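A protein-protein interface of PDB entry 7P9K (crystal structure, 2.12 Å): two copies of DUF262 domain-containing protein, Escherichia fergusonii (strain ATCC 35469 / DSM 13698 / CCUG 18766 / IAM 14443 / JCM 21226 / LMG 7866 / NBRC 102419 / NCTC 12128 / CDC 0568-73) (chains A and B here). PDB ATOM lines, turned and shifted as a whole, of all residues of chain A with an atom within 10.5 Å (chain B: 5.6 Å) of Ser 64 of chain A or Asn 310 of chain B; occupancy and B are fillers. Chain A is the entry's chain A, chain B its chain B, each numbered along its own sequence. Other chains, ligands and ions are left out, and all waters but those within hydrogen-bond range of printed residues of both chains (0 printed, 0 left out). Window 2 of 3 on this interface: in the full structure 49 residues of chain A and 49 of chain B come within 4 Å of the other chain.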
ATOM      1  N   PRO A  23      14.031  10.693 -27.561  1.00  0.00           N
ATOM      2  CA  PRO A  23      13.223   9.992 -26.559  1.00  0.00           C
ATOM      3  C   PRO A  23      13.535  10.537 -25.166  1.00  0.00           C
ATOM      4  O   PRO A  23      14.619  11.062 -24.909  1.00  0.00           O
ATOM      5  CB  PRO A  23      13.664   8.537 -26.720  1.00  0.00           C
ATOM      6  CG  PRO A  23      15.126   8.683 -27.084  1.00  0.00           C
ATOM      7  CD  PRO A  23      15.159   9.868 -28.021  1.00  0.00           C
ATOM      8  N   ALA A  24      12.567  10.414 -24.259  1.00  0.00           N
ATOM      9  CA  ALA A  24      12.630  11.142 -22.993  1.00  0.00           C
ATOM     10  C   ALA A  24      13.960  11.015 -22.253  1.00  0.00           C
ATOM     11  O   ALA A  24      14.302  11.911 -21.470  1.00  0.00           O
ATOM     12  CB  ALA A  24      11.507  10.682 -22.066  1.00  0.00           C
ATOM     13  N   TRP A  55      15.192   5.571 -34.447  1.00  0.00           N
ATOM     14  CA  TRP A  55      14.015   4.746 -34.210  1.00  0.00           C
ATOM     15  C   TRP A  55      12.821   5.444 -34.838  1.00  0.00           C
ATOM     16  O   TRP A  55      12.506   6.586 -34.476  1.00  0.00           O
ATOM     17  CB  TRP A  55      13.825   4.543 -32.705  1.00  0.00           C
ATOM     18  CG  TRP A  55      12.517   3.949 -32.262  1.00  0.00           C
ATOM     19  CD1 TRP A  55      11.703   3.088 -32.955  1.00  0.00           C
ATOM     20  CD2 TRP A  55      11.884   4.172 -31.005  1.00  0.00           C
ATOM     21  NE1 TRP A  55      10.598   2.775 -32.200  1.00  0.00           N
ATOM     22  CE2 TRP A  55      10.690   3.425 -30.997  1.00  0.00           C
ATOM     23  CE3 TRP A  55      12.214   4.928 -29.885  1.00  0.00           C
ATOM     24  CZ2 TRP A  55       9.828   3.424 -29.917  1.00  0.00           C
ATOM     25  CZ3 TRP A  55      11.362   4.918 -28.816  1.00  0.00           C
ATOM     26  CH2 TRP A  55      10.180   4.175 -28.836  1.00  0.00           C
ATOM     27  N   LYS A  56      12.165   4.773 -35.780  1.00  0.00           N
ATOM     28  CA  LYS A  56      11.051   5.384 -36.494  1.00  0.00           C
ATOM     29  C   LYS A  56       9.758   5.216 -35.712  1.00  0.00           C
ATOM     30  O   LYS A  56       9.402   4.104 -35.309  1.00  0.00           O
ATOM     31  CB  LYS A  56      10.905   4.777 -37.885  1.00  0.00           C
ATOM     32  CG  LYS A  56      12.075   5.081 -38.785  1.00  0.00           C
ATOM     33  CD  LYS A  56      12.405   3.905 -39.691  1.00  0.00           C
ATOM     34  CE  LYS A  56      11.231   3.576 -40.605  1.00  0.00           C
ATOM     35  NZ  LYS A  56      10.768   4.775 -41.365  1.00  0.00           N
ATOM     36  N   ILE A  57       9.052   6.321 -35.498  1.00  0.00           N
ATOM     37  CA  ILE A  57       7.784   6.314 -34.784  1.00  0.00           C
ATOM     38  C   ILE A  57       6.677   6.493 -35.818  1.00  0.00           C
ATOM     39  O   ILE A  57       6.589   7.536 -36.479  1.00  0.00           O
ATOM     40  CB  ILE A  57       7.725   7.410 -33.715  1.00  0.00           C
ATOM     41  CG1 ILE A  57       9.057   7.506 -32.953  1.00  0.00           C
ATOM     42  CG2 ILE A  57       6.545   7.185 -32.802  1.00  0.00           C
ATOM     43  CD1 ILE A  57       9.533   6.210 -32.365  1.00  0.00           C
ATOM     44  N   LYS A  58       5.832   5.475 -35.967  1.00  0.00           N
ATOM     45  CA  LYS A  58       4.714   5.585 -36.889  1.00  0.00           C
ATOM     46  C   LYS A  58       3.679   6.559 -36.324  1.00  0.00           C
ATOM     47  O   LYS A  58       3.560   6.719 -35.103  1.00  0.00           O
ATOM     48  CB  LYS A  58       4.092   4.215 -37.154  1.00  0.00           C
ATOM     49  CG  LYS A  58       5.078   3.244 -37.825  1.00  0.00           C
ATOM     50  CD  LYS A  58       4.399   2.036 -38.471  1.00  0.00           C
ATOM     51  CE  LYS A  58       5.361   1.301 -39.407  1.00  0.00           C
ATOM     52  NZ  LYS A  58       4.657   0.546 -40.499  1.00  0.00           N
ATOM     53  N   PRO A  59       2.945   7.252 -37.193  1.00  0.00           N
ATOM     54  CA  PRO A  59       2.054   8.316 -36.703  1.00  0.00           C
ATOM     55  C   PRO A  59       1.046   7.824 -35.683  1.00  0.00           C
ATOM     56  O   PRO A  59       0.632   8.594 -34.808  1.00  0.00           O
ATOM     57  CB  PRO A  59       1.370   8.821 -37.984  1.00  0.00           C
ATOM     58  CG  PRO A  59       2.210   8.312 -39.112  1.00  0.00           C
ATOM     59  CD  PRO A  59       2.793   7.020 -38.639  1.00  0.00           C
ATOM     60  N   GLU A  60       0.651   6.550 -35.760  1.00  0.00           N
ATOM     61  CA  GLU A  60      -0.257   5.973 -34.774  1.00  0.00           C
ATOM     62  C   GLU A  60       0.315   5.980 -33.359  1.00  0.00           C
ATOM     63  O   GLU A  60      -0.450   5.887 -32.393  1.00  0.00           O
ATOM     64  CB  GLU A  60      -0.608   4.546 -35.185  1.00  0.00           C
ATOM     65  CG  GLU A  60       0.540   3.822 -35.850  1.00  0.00           C
ATOM     66  CD  GLU A  60       0.335   2.319 -35.895  1.00  0.00           C
ATOM     67  OE1 GLU A  60       0.976   1.596 -35.093  1.00  0.00           O
ATOM     68  OE2 GLU A  60      -0.467   1.861 -36.741  1.00  0.00           O
ATOM     69  N   ASN A  61       1.635   6.081 -33.199  1.00  0.00           N
ATOM     70  CA  ASN A  61       2.245   6.079 -31.871  1.00  0.00           C
ATOM     71  C   ASN A  61       2.873   7.414 -31.514  1.00  0.00           C
ATOM     72  O   ASN A  61       3.634   7.487 -30.546  1.00  0.00           O
ATOM     73  CB  ASN A  61       3.285   4.966 -31.766  1.00  0.00           C
ATOM     74  CG  ASN A  61       2.758   3.644 -32.281  1.00  0.00           C
ATOM     75  OD1 ASN A  61       3.435   2.934 -33.042  1.00  0.00           O
ATOM     76  ND2 ASN A  61       1.530   3.308 -31.882  1.00  0.00           N
ATOM     77  N   ARG A  62       2.581   8.467 -32.272  1.00  0.00           N
ATOM     78  CA  ARG A  62       3.187   9.759 -31.978  1.00  0.00           C
ATOM     79  C   ARG A  62       2.875  10.231 -30.565  1.00  0.00           C
ATOM     80  O   ARG A  62       3.594  11.085 -30.039  1.00  0.00           O
ATOM     81  CB  ARG A  62       2.728  10.801 -33.003  1.00  0.00           C
ATOM     82  CG  ARG A  62       1.229  10.804 -33.250  1.00  0.00           C
ATOM     83  CD  ARG A  62       0.856  11.621 -34.493  1.00  0.00           C
ATOM     84  NE  ARG A  62       1.134  13.043 -34.306  1.00  0.00           N
ATOM     85  CZ  ARG A  62       0.314  13.886 -33.691  1.00  0.00           C
ATOM     86  NH1 ARG A  62       0.653  15.162 -33.559  1.00  0.00           N
ATOM     87  NH2 ARG A  62      -0.842  13.450 -33.205  1.00  0.00           N
ATOM     88  N   ASP A  63       1.836   9.693 -29.931  1.00  0.00           N
ATOM     89  CA  ASP A  63       1.454  10.090 -28.578  1.00  0.00           C
ATOM     90  C   ASP A  63       1.843   9.066 -27.517  1.00  0.00           C
ATOM     91  O   ASP A  63       1.672   9.334 -26.325  1.00  0.00           O
ATOM     92  CB  ASP A  63      -0.060  10.345 -28.510  1.00  0.00           C
ATOM     93  CG  ASP A  63      -0.460  11.693 -29.099  1.00  0.00           C
ATOM     94  OD1 ASP A  63      -0.159  12.732 -28.463  1.00  0.00           O
ATOM     95  OD2 ASP A  63      -1.085  11.714 -30.188  1.00  0.00           O
ATOM     96  N   SER A  64       2.371   7.909 -27.922  1.00  0.00           N
ATOM     97  CA  SER A  64       2.628   6.816 -26.995  1.00  0.00           C
ATOM     98  C   SER A  64       3.813   7.076 -26.083  1.00  0.00           C
ATOM     99  O   SER A  64       3.964   6.382 -25.071  1.00  0.00           O
ATOM    100  CB  SER A  64       2.873   5.514 -27.760  1.00  0.00           C
ATOM    101  OG  SER A  64       1.911   5.304 -28.771  1.00  0.00           O
ATOM    102  N   TYR A  65       4.666   8.041 -26.412  1.00  0.00           N
ATOM    103  CA  TYR A  65       5.876   8.246 -25.635  1.00  0.00           C
ATOM    104  C   TYR A  65       6.127   9.737 -25.490  1.00  0.00           C
ATOM    105  O   TYR A  65       5.574  10.546 -26.230  1.00  0.00           O
ATOM    106  CB  TYR A  65       7.087   7.554 -26.283  1.00  0.00           C
ATOM    107  CG  TYR A  65       6.828   6.143 -26.795  1.00  0.00           C
ATOM    108  CD1 TYR A  65       6.913   5.044 -25.933  1.00  0.00           C
ATOM    109  CD2 TYR A  65       6.519   5.904 -28.137  1.00  0.00           C
ATOM    110  CE1 TYR A  65       6.675   3.758 -26.387  1.00  0.00           C
ATOM    111  CE2 TYR A  65       6.280   4.601 -28.606  1.00  0.00           C
ATOM    112  CZ  TYR A  65       6.365   3.537 -27.714  1.00  0.00           C
ATOM    113  OH  TYR A  65       6.145   2.243 -28.135  1.00  0.00           O
ATOM    114  N   GLN A  66       6.980  10.089 -24.532  1.00  0.00           N
ATOM    115  CA  GLN A  66       7.403  11.470 -24.339  1.00  0.00           C
ATOM    116  C   GLN A  66       8.673  11.754 -25.142  1.00  0.00           C
ATOM    117  O   GLN A  66       9.658  11.019 -25.030  1.00  0.00           O
ATOM    118  CB  GLN A  66       7.650  11.740 -22.853  1.00  0.00           C
ATOM    119  CG  GLN A  66       7.797  13.203 -22.518  1.00  0.00           C
ATOM    120  CD  GLN A  66       6.673  14.030 -23.106  1.00  0.00           C
ATOM    121  OE1 GLN A  66       5.494  13.738 -22.889  1.00  0.00           O
ATOM    122  NE2 GLN A  66       7.032  15.066 -23.868  1.00  0.00           N
ATOM    123  N   PHE A  67       8.657  12.831 -25.929  1.00  0.00           N
ATOM    124  CA  PHE A  67       9.807  13.242 -26.725  1.00  0.00           C
ATOM    125  C   PHE A  67      10.252  14.646 -26.358  1.00  0.00           C
ATOM    126  O   PHE A  67       9.503  15.426 -25.765  1.00  0.00           O
ATOM    127  CB  PHE A  67       9.498  13.212 -28.217  1.00  0.00           C
ATOM    128  CG  PHE A  67       9.120  11.869 -28.715  1.00  0.00           C
ATOM    129  CD1 PHE A  67      10.097  10.896 -28.939  1.00  0.00           C
ATOM    130  CD2 PHE A  67       7.795  11.564 -28.961  1.00  0.00           C
ATOM    131  CE1 PHE A  67       9.752   9.641 -29.411  1.00  0.00           C
ATOM    132  CE2 PHE A  67       7.437  10.315 -29.425  1.00  0.00           C
ATOM    133  CZ  PHE A  67       8.417   9.343 -29.647  1.00  0.00           C
ATOM    134  N   LEU A  88       4.498  18.621 -32.964  1.00  0.00           N
ATOM    135  CA  LEU A  88       4.748  17.184 -33.108  1.00  0.00           C
ATOM    136  C   LEU A  88       4.431  16.750 -34.536  1.00  0.00           C
ATOM    137  O   LEU A  88       3.333  17.018 -35.026  1.00  0.00           O
ATOM    138  CB  LEU A  88       3.925  16.362 -32.114  1.00  0.00           C
ATOM    139  CG  LEU A  88       4.300  14.874 -31.979  1.00  0.00           C
ATOM    140  CD1 LEU A  88       5.620  14.674 -31.220  1.00  0.00           C
ATOM    141  CD2 LEU A  88       3.184  14.061 -31.319  1.00  0.00           C
ATOM    142  N   PRO A  89       5.343  16.061 -35.220  1.00  0.00           N
ATOM    143  CA  PRO A  89       5.051  15.609 -36.587  1.00  0.00           C
ATOM    144  C   PRO A  89       3.791  14.758 -36.650  1.00  0.00           C
ATOM    145  O   PRO A  89       3.507  13.963 -35.752  1.00  0.00           O
ATOM    146  CB  PRO A  89       6.301  14.801 -36.960  1.00  0.00           C
ATOM    147  CG  PRO A  89       7.399  15.353 -36.046  1.00  0.00           C
ATOM    148  CD  PRO A  89       6.693  15.663 -34.774  1.00  0.00           C
ATOM    149  N   PHE A  93       8.186  10.011 -38.042  1.00  0.00           N
ATOM    150  CA  PHE A  93       9.320  10.809 -37.590  1.00  0.00           C
ATOM    151  C   PHE A  93      10.322   9.911 -36.854  1.00  0.00           C
ATOM    152  O   PHE A  93      10.159   8.689 -36.777  1.00  0.00           O
ATOM    153  CB  PHE A  93       8.869  12.003 -36.725  1.00  0.00           C
ATOM    154  CG  PHE A  93       8.264  11.629 -35.387  1.00  0.00           C
ATOM    155  CD1 PHE A  93       6.914  11.317 -35.274  1.00  0.00           C
ATOM    156  CD2 PHE A  93       9.033  11.651 -34.237  1.00  0.00           C
ATOM    157  CE1 PHE A  93       6.346  10.994 -34.034  1.00  0.00           C
ATOM    158  CE2 PHE A  93       8.472  11.336 -32.993  1.00  0.00           C
ATOM    159  CZ  PHE A  93       7.126  11.003 -32.895  1.00  0.00           C
ATOM    160  N   ASP A 225       9.484  -0.304 -34.535  1.00  0.00           N
ATOM    161  CA  ASP A 225       9.312  -1.147 -33.352  1.00  0.00           C
ATOM    162  C   ASP A 225       9.712  -2.588 -33.631  1.00  0.00           C
ATOM    163  O   ASP A 225      10.384  -3.225 -32.811  1.00  0.00           O
ATOM    164  CB  ASP A 225       7.855  -1.118 -32.871  1.00  0.00           C
ATOM    165  CG  ASP A 225       7.386   0.263 -32.469  1.00  0.00           C
ATOM    166  OD1 ASP A 225       8.017   1.266 -32.881  1.00  0.00           O
ATOM    167  OD2 ASP A 225       6.366   0.346 -31.743  1.00  0.00           O
ATOM    168  N   GLN B 258       7.223   7.747 -18.227  1.00  0.00           N
ATOM    169  CA  GLN B 258       5.784   7.961 -18.201  1.00  0.00           C
ATOM    170  C   GLN B 258       5.191   8.093 -16.792  1.00  0.00           C
ATOM    171  O   GLN B 258       3.978   7.923 -16.639  1.00  0.00           O
ATOM    172  CB  GLN B 258       5.081   6.827 -18.943  1.00  0.00           C
ATOM    173  CG  GLN B 258       5.729   6.421 -20.246  1.00  0.00           C
ATOM    174  CD  GLN B 258       5.642   7.499 -21.317  1.00  0.00           C
ATOM    175  OE1 GLN B 258       4.933   8.511 -21.155  1.00  0.00           O
ATOM    176  NE2 GLN B 258       6.359   7.283 -22.432  1.00  0.00           N
ATOM    177  N   VAL B 306       9.257  -2.505 -26.517  1.00  0.00           N
ATOM    178  CA  VAL B 306       9.116  -1.081 -26.216  1.00  0.00           C
ATOM    179  C   VAL B 306       7.663  -0.644 -26.376  1.00  0.00           C
ATOM    180  O   VAL B 306       7.159   0.175 -25.598  1.00  0.00           O
ATOM    181  CB  VAL B 306      10.065  -0.250 -27.100  1.00  0.00           C
ATOM    182  CG1 VAL B 306       9.629  -0.302 -28.566  1.00  0.00           C
ATOM    183  CG2 VAL B 306      10.148   1.174 -26.602  1.00  0.00           C
ATOM    184  N   GLU B 307       6.957  -1.201 -27.367  1.00  0.00           N
ATOM    185  CA  GLU B 307       5.573  -0.807 -27.615  1.00  0.00           C
ATOM    186  C   GLU B 307       4.665  -1.048 -26.412  1.00  0.00           C
ATOM    187  O   GLU B 307       3.629  -0.387 -26.287  1.00  0.00           O
ATOM    188  CB  GLU B 307       5.024  -1.558 -28.821  1.00  0.00           C
ATOM    189  CG  GLU B 307       5.371  -3.043 -28.838  1.00  0.00           C
ATOM    190  CD  GLU B 307       6.625  -3.364 -29.673  1.00  0.00           C
ATOM    191  OE1 GLU B 307       7.682  -2.720 -29.439  1.00  0.00           O
ATOM    192  OE2 GLU B 307       6.544  -4.255 -30.560  1.00  0.00           O
ATOM    193  N   ASN B 308       5.020  -1.979 -25.528  1.00  0.00           N
ATOM    194  CA  ASN B 308       4.194  -2.282 -24.367  1.00  0.00           C
ATOM    195  C   ASN B 308       4.376  -1.289 -23.244  1.00  0.00           C
ATOM    196  O   ASN B 308       3.563  -1.277 -22.314  1.00  0.00           O
ATOM    197  CB  ASN B 308       4.503  -3.684 -23.836  1.00  0.00           C
ATOM    198  CG  ASN B 308       3.936  -4.754 -24.716  1.00  0.00           C
ATOM    199  OD1 ASN B 308       3.099  -4.473 -25.575  1.00  0.00           O
ATOM    200  ND2 ASN B 308       4.385  -5.988 -24.524  1.00  0.00           N
ATOM    201  N   PHE B 309       5.425  -0.476 -23.304  1.00  0.00           N
ATOM    202  CA  PHE B 309       5.718   0.498 -22.264  1.00  0.00           C
ATOM    203  C   PHE B 309       5.340   1.903 -22.714  1.00  0.00           C
ATOM    204  O   PHE B 309       6.058   2.876 -22.483  1.00  0.00           O
ATOM    205  CB  PHE B 309       7.183   0.384 -21.857  1.00  0.00           C
ATOM    206  CG  PHE B 309       7.497  -0.936 -21.201  1.00  0.00           C
ATOM    207  CD1 PHE B 309       7.285  -1.118 -19.852  1.00  0.00           C
ATOM    208  CD2 PHE B 309       7.918  -2.017 -21.953  1.00  0.00           C
ATOM    209  CE1 PHE B 309       7.526  -2.351 -19.256  1.00  0.00           C
ATOM    210  CE2 PHE B 309       8.166  -3.245 -21.365  1.00  0.00           C
ATOM    211  CZ  PHE B 309       7.959  -3.417 -20.019  1.00  0.00           C
ATOM    212  N   ASN B 310       4.192   2.000 -23.374  1.00  0.00           N
ATOM    213  CA  ASN B 310       3.613   3.263 -23.790  1.00  0.00           C
ATOM    214  C   ASN B 310       2.986   3.942 -22.580  1.00  0.00           C
ATOM    215  O   ASN B 310       2.994   3.413 -21.461  1.00  0.00           O
ATOM    216  CB  ASN B 310       2.607   3.041 -24.919  1.00  0.00           C
ATOM    217  CG  ASN B 310       1.490   2.089 -24.534  1.00  0.00           C
ATOM    218  OD1 ASN B 310       1.062   2.028 -23.375  1.00  0.00           O
ATOM    219  ND2 ASN B 310       1.004   1.345 -25.507  1.00  0.00           N
ATOM    220  N   LYS B 311       2.447   5.139 -22.782  1.00  0.00           N
ATOM    221  CA  LYS B 311       2.092   5.920 -21.605  1.00  0.00           C
ATOM    222  C   LYS B 311       0.796   5.435 -20.965  1.00  0.00           C
ATOM    223  O   LYS B 311       0.634   5.562 -19.749  1.00  0.00           O
ATOM    224  CB  LYS B 311       2.035   7.412 -21.952  1.00  0.00           C
ATOM    225  CG  LYS B 311       0.865   7.863 -22.818  1.00  0.00           C
ATOM    226  CD  LYS B 311       0.660   9.377 -22.671  1.00  0.00           C
ATOM    227  CE  LYS B 311       2.000  10.138 -22.684  1.00  0.00           C
ATOM    228  NZ  LYS B 311       2.509  10.437 -24.068  1.00  0.00           N
ATOM    229  N   GLU B 312      -0.116   4.839 -21.729  1.00  0.00           N
ATOM    230  CA  GLU B 312      -1.323   4.329 -21.090  1.00  0.00           C
ATOM    231  C   GLU B 312      -1.015   3.124 -20.206  1.00  0.00           C
ATOM    232  O   GLU B 312      -1.544   3.020 -19.088  1.00  0.00           O
ATOM    233  CB  GLU B 312      -2.371   3.981 -22.133  1.00  0.00           C
ATOM    234  CG  GLU B 312      -1.842   3.245 -23.321  1.00  0.00           C
ATOM    235  CD  GLU B 312      -2.894   2.325 -23.941  1.00  0.00           C
ATOM    236  OE1 GLU B 312      -2.496   1.323 -24.590  1.00  0.00           O
ATOM    237  OE2 GLU B 312      -4.110   2.600 -23.782  1.00  0.00           O
ATOM    238  N   ASN B 313      -0.148   2.211 -20.676  1.00  0.00           N
ATOM    239  CA  ASN B 313       0.207   1.041 -19.877  1.00  0.00           C
ATOM    240  C   ASN B 313       1.028   1.429 -18.659  1.00  0.00           C
ATOM    241  O   ASN B 313       0.879   0.833 -17.584  1.00  0.00           O
ATOM    242  CB  ASN B 313       0.986   0.036 -20.709  1.00  0.00           C
ATOM    243  CG  ASN B 313       0.142  -0.676 -21.731  1.00  0.00           C
ATOM    244  OD1 ASN B 313      -1.078  -0.538 -21.763  1.00  0.00           O
ATOM    245  ND2 ASN B 313       0.798  -1.471 -22.572  1.00  0.00           N
ATOM    246  N   MET B 314       1.933   2.394 -18.812  1.00  0.00           N
ATOM    247  CA  MET B 314       2.690   2.837 -17.656  1.00  0.00           C
ATOM    248  C   MET B 314       1.817   3.597 -16.660  1.00  0.00           C
ATOM    249  O   MET B 314       2.187   3.714 -15.491  1.00  0.00           O
ATOM    250  CB  MET B 314       3.867   3.692 -18.108  1.00  0.00           C
ATOM    251  CG  MET B 314       4.962   2.890 -18.817  1.00  0.00           C
ATOM    252  SD  MET B 314       5.544   1.520 -17.797  1.00  0.00           S
ATOM    253  CE  MET B 314       4.657   0.148 -18.542  1.00  0.00           C
ATOM    254  N   ALA B 315       0.670   4.116 -17.102  1.00  0.00           N
ATOM    255  CA  ALA B 315      -0.274   4.739 -16.179  1.00  0.00           C
ATOM    256  C   ALA B 315      -0.960   3.684 -15.324  1.00  0.00           C
ATOM    257  O   ALA B 315      -1.113   3.859 -14.111  1.00  0.00           O
ATOM    258  CB  ALA B 315      -1.307   5.560 -16.949  1.00  0.00           C
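NZ of Lys 311 of chain B is in hydrogen-bond range of O of Asp 63 of chain A (2.6 Å).
N of Lys 311 of chain B sits at hydrogen-bond distance from O of Ser 64 of chain A.
The backbone carbonyl oxygen of Val 306 of chain B lies within hydrogen-bond range of the side-chain hydroxyl of Tyr 65 of chain A (3.4 Å).
No position is printed for both chains.
Of the 11 pairs that touch across the chains among the printed residues, none has its exchanged pair printed and touching as well.
Val 306 of chain B touches Trp 55 of chain A.
NE2 of Gln 258 of chain B touches O of Ser 64 of chain A (3.7 Å).
Ser 64 of chain A touches Asn 310 of chain B.
Tyr 65 of chain A touches Gln 258 of chain B (CA to NE2, 3.4 Å).
Glu 307 of chain B touches Tyr 65 of chain A.
Tyr 65 of chain A touches Lys 311 of chain B.
NE2 of Gln 258 of chain B touches N of Gln 66 of chain A (3.6 Å).
Glu 307 of chain B touches Asp 225 of chain A (CB to OD2, 3.7 Å).
Printed residues of chain B that touch a printed residue of chain A: Gln 258, Val 306, Glu 307, Asn 310 and Lys 311.
Hydrophobic or aromatic side chains of chain B that line the printed part of chain A: Val 306.
Of the 19 printed residues of chain A, 6 touch a printed residue of chain B.
Hydrophobic or aromatic side chains of chain A that line the printed part of chain B: Trp 55 and Tyr 65.
Printed residues of chain B within 4 Å of Trp 55 of chain A: Val 306 (3.7 Å).
Of chain B, only Gln 258 (3.7 Å), Asn 310 (3.4 Å) and Lys 311 (3.0 Å) come within 4 Å of Ser 64 of chain A.
Of the printed residues of chain A, Val 306 of chain B touches Trp 55 (3.7 Å) and Tyr 65 (3.4 Å).
Of chain A, only Ser 64 (3.4 Å) comes within 4 Å of Asn 310 of chain B.
Lys 311 of chain B touches three residues of chain A.
Asn 313 of chain B touches none of the printed residues of chain A.
Met 314 of chain B touches none of the printed residues of chain A.
The nearest residue of chain B that does not touch Ser 64 of chain A is Phe 309 of chain B (4.8 Å).
The nearest residue of chain A that does not touch Asn 310 of chain B is Tyr 65 of chain A (4.05 Å).
The backbone NH of Ala 24 of chain A sits at hydrogen-bond distance from the backbone carbonyl oxygen of Gln 66 of chain A (3.1 Å).
The backbone carbonyl oxygen (O) of Asn 61 of chain A sits close to the side-chain hydroxyl (OG) of Ser 64 of chain A (3.3 Å).
OD2 of Asp 63 of chain A lies within salt-bridge range of NH2 of Arg 62 of chain A (3.5 Å).
The backbone carbonyl oxygen of Glu 307 of chain B sits at hydrogen-bond distance from the side-chain amide nitrogen of Asn 310 of chain B (3.2 Å).
The backbone NH (N) of Glu 312 of chain B sits close to the side-chain amide oxygen (OD1) of Asn 310 of chain B.
The backbone NH (N) of Asn 313 of chain B lies within hydrogen-bond range of the side-chain amide oxygen (OD1) of Asn 310 of chain B.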
